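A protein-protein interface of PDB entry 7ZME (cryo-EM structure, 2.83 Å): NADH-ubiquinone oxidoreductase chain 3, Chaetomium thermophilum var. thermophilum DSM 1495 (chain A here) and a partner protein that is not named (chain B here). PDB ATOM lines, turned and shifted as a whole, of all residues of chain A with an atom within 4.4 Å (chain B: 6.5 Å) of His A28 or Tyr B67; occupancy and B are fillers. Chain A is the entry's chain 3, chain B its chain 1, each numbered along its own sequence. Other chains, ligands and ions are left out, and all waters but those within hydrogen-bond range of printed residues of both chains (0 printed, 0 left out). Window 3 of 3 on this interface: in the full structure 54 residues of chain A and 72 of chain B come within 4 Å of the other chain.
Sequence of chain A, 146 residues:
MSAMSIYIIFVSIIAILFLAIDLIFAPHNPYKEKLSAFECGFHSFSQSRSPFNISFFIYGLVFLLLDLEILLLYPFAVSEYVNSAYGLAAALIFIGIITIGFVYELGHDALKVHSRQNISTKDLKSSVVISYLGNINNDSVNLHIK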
ATOM      1  N   LEU A  23       5.269  27.070  -2.798  1.00  0.00           N
ATOM      2  CA  LEU A  23       6.649  27.238  -3.234  1.00  0.00           C
ATOM      3  C   LEU A  23       7.561  27.783  -2.145  1.00  0.00           C
ATOM      4  O   LEU A  23       8.780  27.800  -2.339  1.00  0.00           O
ATOM      5  CB  LEU A  23       6.705  28.157  -4.453  1.00  0.00           C
ATOM      6  CG  LEU A  23       6.319  27.526  -5.789  1.00  0.00           C
ATOM      7  CD1 LEU A  23       5.983  28.604  -6.803  1.00  0.00           C
ATOM      8  CD2 LEU A  23       7.439  26.638  -6.302  1.00  0.00           C
ATOM      9  N   ALA A  26       6.340  24.755   1.787  1.00  0.00           N
ATOM     10  CA  ALA A  26       6.305  23.310   1.792  1.00  0.00           C
ATOM     11  C   ALA A  26       7.718  22.750   1.736  1.00  0.00           C
ATOM     12  O   ALA A  26       8.615  23.383   1.175  1.00  0.00           O
ATOM     13  CB  ALA A  26       5.500  22.761   0.610  1.00  0.00           C
ATOM     14  N   PRO A  27       7.953  21.577   2.319  1.00  0.00           N
ATOM     15  CA  PRO A  27       9.254  20.924   2.154  1.00  0.00           C
ATOM     16  C   PRO A  27       9.510  20.594   0.694  1.00  0.00           C
ATOM     17  O   PRO A  27       8.584  20.369  -0.085  1.00  0.00           O
ATOM     18  CB  PRO A  27       9.123  19.655   3.002  1.00  0.00           C
ATOM     19  CG  PRO A  27       7.650  19.443   3.144  1.00  0.00           C
ATOM     20  CD  PRO A  27       7.061  20.806   3.201  1.00  0.00           C
ATOM     21  N   HIS A  28      10.785  20.590   0.318  1.00  0.00           N
ATOM     22  CA  HIS A  28      11.184  20.271  -1.050  1.00  0.00           C
ATOM     23  C   HIS A  28      12.448  19.429  -1.001  1.00  0.00           C
ATOM     24  O   HIS A  28      13.533  19.949  -0.728  1.00  0.00           O
ATOM     25  CB  HIS A  28      11.402  21.535  -1.877  1.00  0.00           C
ATOM     26  CG  HIS A  28      11.309  21.304  -3.352  1.00  0.00           C
ATOM     27  ND1 HIS A  28      12.418  21.222  -4.162  1.00  0.00           N
ATOM     28  CD2 HIS A  28      10.239  21.114  -4.157  1.00  0.00           C
ATOM     29  CE1 HIS A  28      12.035  21.003  -5.407  1.00  0.00           C
ATOM     30  NE2 HIS A  28      10.716  20.932  -5.430  1.00  0.00           N
ATOM     31  N   ASN A  29      12.307  18.134  -1.266  1.00  0.00           N
ATOM     32  CA  ASN A  29      13.412  17.177  -1.193  1.00  0.00           C
ATOM     33  C   ASN A  29      13.413  16.320  -2.451  1.00  0.00           C
ATOM     34  O   ASN A  29      13.093  15.127  -2.408  1.00  0.00           O
ATOM     35  CB  ASN A  29      13.292  16.315   0.062  1.00  0.00           C
ATOM     36  CG  ASN A  29      13.554  17.099   1.328  1.00  0.00           C
ATOM     37  OD1 ASN A  29      14.469  17.919   1.385  1.00  0.00           O
ATOM     38  ND2 ASN A  29      12.740  16.862   2.349  1.00  0.00           N
ATOM     39  N   PRO A  30      13.773  16.900  -3.597  1.00  0.00           N
ATOM     40  CA  PRO A  30      13.719  16.143  -4.855  1.00  0.00           C
ATOM     41  C   PRO A  30      14.936  15.243  -5.010  1.00  0.00           C
ATOM     42  O   PRO A  30      16.079  15.700  -4.947  1.00  0.00           O
ATOM     43  CB  PRO A  30      13.694  17.238  -5.924  1.00  0.00           C
ATOM     44  CG  PRO A  30      14.400  18.383  -5.293  1.00  0.00           C
ATOM     45  CD  PRO A  30      14.169  18.303  -3.812  1.00  0.00           C
ATOM     46  N   LYS B  65       1.987  20.703   1.298  1.00  0.00           N
ATOM     47  CA  LYS B  65       2.482  19.416   0.838  1.00  0.00           C
ATOM     48  C   LYS B  65       3.519  19.631  -0.259  1.00  0.00           C
ATOM     49  O   LYS B  65       3.417  20.564  -1.056  1.00  0.00           O
ATOM     50  CB  LYS B  65       1.316  18.568   0.316  1.00  0.00           C
ATOM     51  CG  LYS B  65       1.637  17.170  -0.180  1.00  0.00           C
ATOM     52  CD  LYS B  65       1.987  16.241   0.958  1.00  0.00           C
ATOM     53  CE  LYS B  65       2.170  14.821   0.472  1.00  0.00           C
ATOM     54  NZ  LYS B  65       2.561  13.904   1.575  1.00  0.00           N
ATOM     55  N   GLU B  66       4.585  18.851  -0.259  1.00  0.00           N
ATOM     56  CA  GLU B  66       5.688  19.037  -1.229  1.00  0.00           C
ATOM     57  C   GLU B  66       5.231  18.858  -2.677  1.00  0.00           C
ATOM     58  O   GLU B  66       4.421  17.974  -2.937  1.00  0.00           O
ATOM     59  CB  GLU B  66       6.765  18.013  -0.893  1.00  0.00           C
ATOM     60  CG  GLU B  66       7.853  17.917  -1.935  1.00  0.00           C
ATOM     61  CD  GLU B  66       8.665  16.654  -1.793  1.00  0.00           C
ATOM     62  OE1 GLU B  66       8.178  15.609  -2.232  1.00  0.00           O
ATOM     63  OE2 GLU B  66       9.764  16.725  -1.229  1.00  0.00           O
ATOM     64  N   TYR B  67       5.780  19.653  -3.592  1.00  0.00           N
ATOM     65  CA  TYR B  67       5.463  19.473  -5.027  1.00  0.00           C
ATOM     66  C   TYR B  67       6.617  18.746  -5.697  1.00  0.00           C
ATOM     67  O   TYR B  67       7.764  18.872  -5.286  1.00  0.00           O
ATOM     68  CB  TYR B  67       5.161  20.794  -5.738  1.00  0.00           C
ATOM     69  CG  TYR B  67       6.364  21.582  -6.186  1.00  0.00           C
ATOM     70  CD1 TYR B  67       6.939  21.369  -7.424  1.00  0.00           C
ATOM     71  CD2 TYR B  67       6.922  22.546  -5.367  1.00  0.00           C
ATOM     72  CE1 TYR B  67       8.055  22.077  -7.829  1.00  0.00           C
ATOM     73  CE2 TYR B  67       8.034  23.269  -5.759  1.00  0.00           C
ATOM     74  CZ  TYR B  67       8.600  23.037  -6.997  1.00  0.00           C
ATOM     75  OH  TYR B  67       9.695  23.748  -7.397  1.00  0.00           O
ATOM     76  N   VAL B  68       6.285  17.960  -6.690  1.00  0.00           N
ATOM     77  CA  VAL B  68       7.327  17.213  -7.420  1.00  0.00           C
ATOM     78  C   VAL B  68       7.374  17.667  -8.871  1.00  0.00           C
ATOM     79  O   VAL B  68       6.317  17.843  -9.461  1.00  0.00           O
ATOM     80  CB  VAL B  68       7.078  15.702  -7.330  1.00  0.00           C
ATOM     81  CG1 VAL B  68       7.954  14.907  -8.288  1.00  0.00           C
ATOM     82  CG2 VAL B  68       7.197  15.182  -5.909  1.00  0.00           C
ATOM     83  N   GLY B  69       8.565  17.944  -9.369  1.00  0.00           N
ATOM     84  CA  GLY B  69       8.697  18.246 -10.795  1.00  0.00           C
ATOM     85  C   GLY B  69       9.318  17.061 -11.484  1.00  0.00           C
ATOM     86  O   GLY B  69      10.515  16.816 -11.290  1.00  0.00           O
ATOM     87  N   LEU B  75       8.385  21.051 -17.662  1.00  0.00           N
ATOM     88  CA  LEU B  75       8.039  21.663 -16.381  1.00  0.00           C
ATOM     89  C   LEU B  75       7.245  22.953 -16.537  1.00  0.00           C
ATOM     90  O   LEU B  75       6.315  23.200 -15.763  1.00  0.00           O
ATOM     91  CB  LEU B  75       9.294  21.927 -15.549  1.00  0.00           C
ATOM     92  CG  LEU B  75       9.859  20.772 -14.718  1.00  0.00           C
ATOM     93  CD1 LEU B  75       8.837  20.324 -13.684  1.00  0.00           C
ATOM     94  CD2 LEU B  75      10.331  19.605 -15.564  1.00  0.00           C
ATOM     95  N   PHE B  79       3.093  23.304 -15.067  1.00  0.00           N
ATOM     96  CA  PHE B  79       2.520  24.295 -14.135  1.00  0.00           C
ATOM     97  C   PHE B  79       1.551  25.189 -14.903  1.00  0.00           C
ATOM     98  O   PHE B  79       0.609  25.694 -14.296  1.00  0.00           O
ATOM     99  CB  PHE B  79       3.628  25.080 -13.434  1.00  0.00           C
ATOM    100  CG  PHE B  79       4.321  24.331 -12.326  1.00  0.00           C
ATOM    101  CD1 PHE B  79       5.198  23.298 -12.606  1.00  0.00           C
ATOM    102  CD2 PHE B  79       4.097  24.663 -11.001  1.00  0.00           C
ATOM    103  CE1 PHE B  79       5.828  22.607 -11.584  1.00  0.00           C
ATOM    104  CE2 PHE B  79       4.726  23.972  -9.979  1.00  0.00           C
ATOM    105  CZ  PHE B  79       5.592  22.946 -10.275  1.00  0.00           C
ATOM    106  N   ALA B 225       0.670  17.103  -8.069  1.00  0.00           N
ATOM    107  CA  ALA B 225       0.604  16.946  -6.599  1.00  0.00           C
ATOM    108  C   ALA B 225       0.541  18.322  -5.938  1.00  0.00           C
ATOM    109  O   ALA B 225       0.692  19.317  -6.668  1.00  0.00           O
ATOM    110  CB  ALA B 225       1.831  16.206  -6.137  1.00  0.00           C
ATOM    111  N   ALA B 226       0.259  18.374  -4.630  1.00  0.00           N
ATOM    112  CA  ALA B 226       0.254  19.640  -3.859  1.00  0.00           C
ATOM    113  C   ALA B 226      -0.723  20.677  -4.432  1.00  0.00           C
ATOM    114  O   ALA B 226      -1.893  20.320  -4.632  1.00  0.00           O
ATOM    115  CB  ALA B 226       1.656  20.169  -3.754  1.00  0.00           C
ATOM    116  N   VAL B 227      -0.263  21.915  -4.659  1.00  0.00           N
ATOM    117  CA  VAL B 227      -1.149  23.025  -5.128  1.00  0.00           C
ATOM    118  C   VAL B 227      -1.556  22.834  -6.599  1.00  0.00           C
ATOM    119  O   VAL B 227      -2.634  23.314  -6.969  1.00  0.00           O
ATOM    120  CB  VAL B 227      -0.509  24.401  -4.858  1.00  0.00           C
ATOM    121  CG1 VAL B 227       0.734  24.637  -5.702  1.00  0.00           C
ATOM    122  CG2 VAL B 227      -1.495  25.543  -5.017  1.00  0.00           C
ATOM    123  N   ILE B 228      -0.734  22.179  -7.413  1.00  0.00           N
ATOM    124  CA  ILE B 228      -1.125  21.873  -8.816  1.00  0.00           C
ATOM    125  C   ILE B 228      -2.365  20.973  -8.786  1.00  0.00           C
ATOM    126  O   ILE B 228      -3.219  21.139  -9.651  1.00  0.00           O
ATOM    127  CB  ILE B 228       0.074  21.259  -9.586  1.00  0.00           C
ATOM    128  CG1 ILE B 228       1.240  22.240  -9.682  1.00  0.00           C
ATOM    129  CG2 ILE B 228      -0.353  20.778 -10.950  1.00  0.00           C
ATOM    130  CD1 ILE B 228       0.852  23.576 -10.258  1.00  0.00           C
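The backbone NH (N) of Asn A29 lies within hydrogen-bond range of the side-chain carboxylate (OE2) of Glu B66, at 2.9 Å.
Among the printed residues, pairs that only touch across the chains: Pro A27 with Glu B66 (3.1 Å), His A28 with Tyr B67 (3.4 Å), Ala A26 with Lys B65 (3.5 Å), Leu A23 with Tyr B67 (3.5 Å) and His A28 with Glu B66 (3.8 Å).
Printed residues of chain B within 4 Å of Leu A23: Tyr B67 (3.5 Å). His A28 touches two residues of chain B. Pro A30 touches none of the printed residues of chain B. Of the printed residues of chain A, Glu B66 touches Pro A27, His A28 and Asn A29. Tyr B67 touches two residues of chain A. Phe B79 touches none of the printed residues of chain A. The nearest printed residue of chain B that does not touch His A28 is Gly B69 (5.4 Å). The nearest printed residue of chain B that does not touch Leu A23 is Phe B79 (5.3 Å).
Hydrophobic or aromatic side chains of chain B within 4 Å of the printed part of chain A: Tyr B67. Along chain B the printed residues that touch a printed residue of chain A span positions 65 to 67. Hydrophobic or aromatic side chains of chain A that line the printed part of chain B: Leu A23, Ala A26 and His A28. Among the printed residues, 6 pairs touch across the chains.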
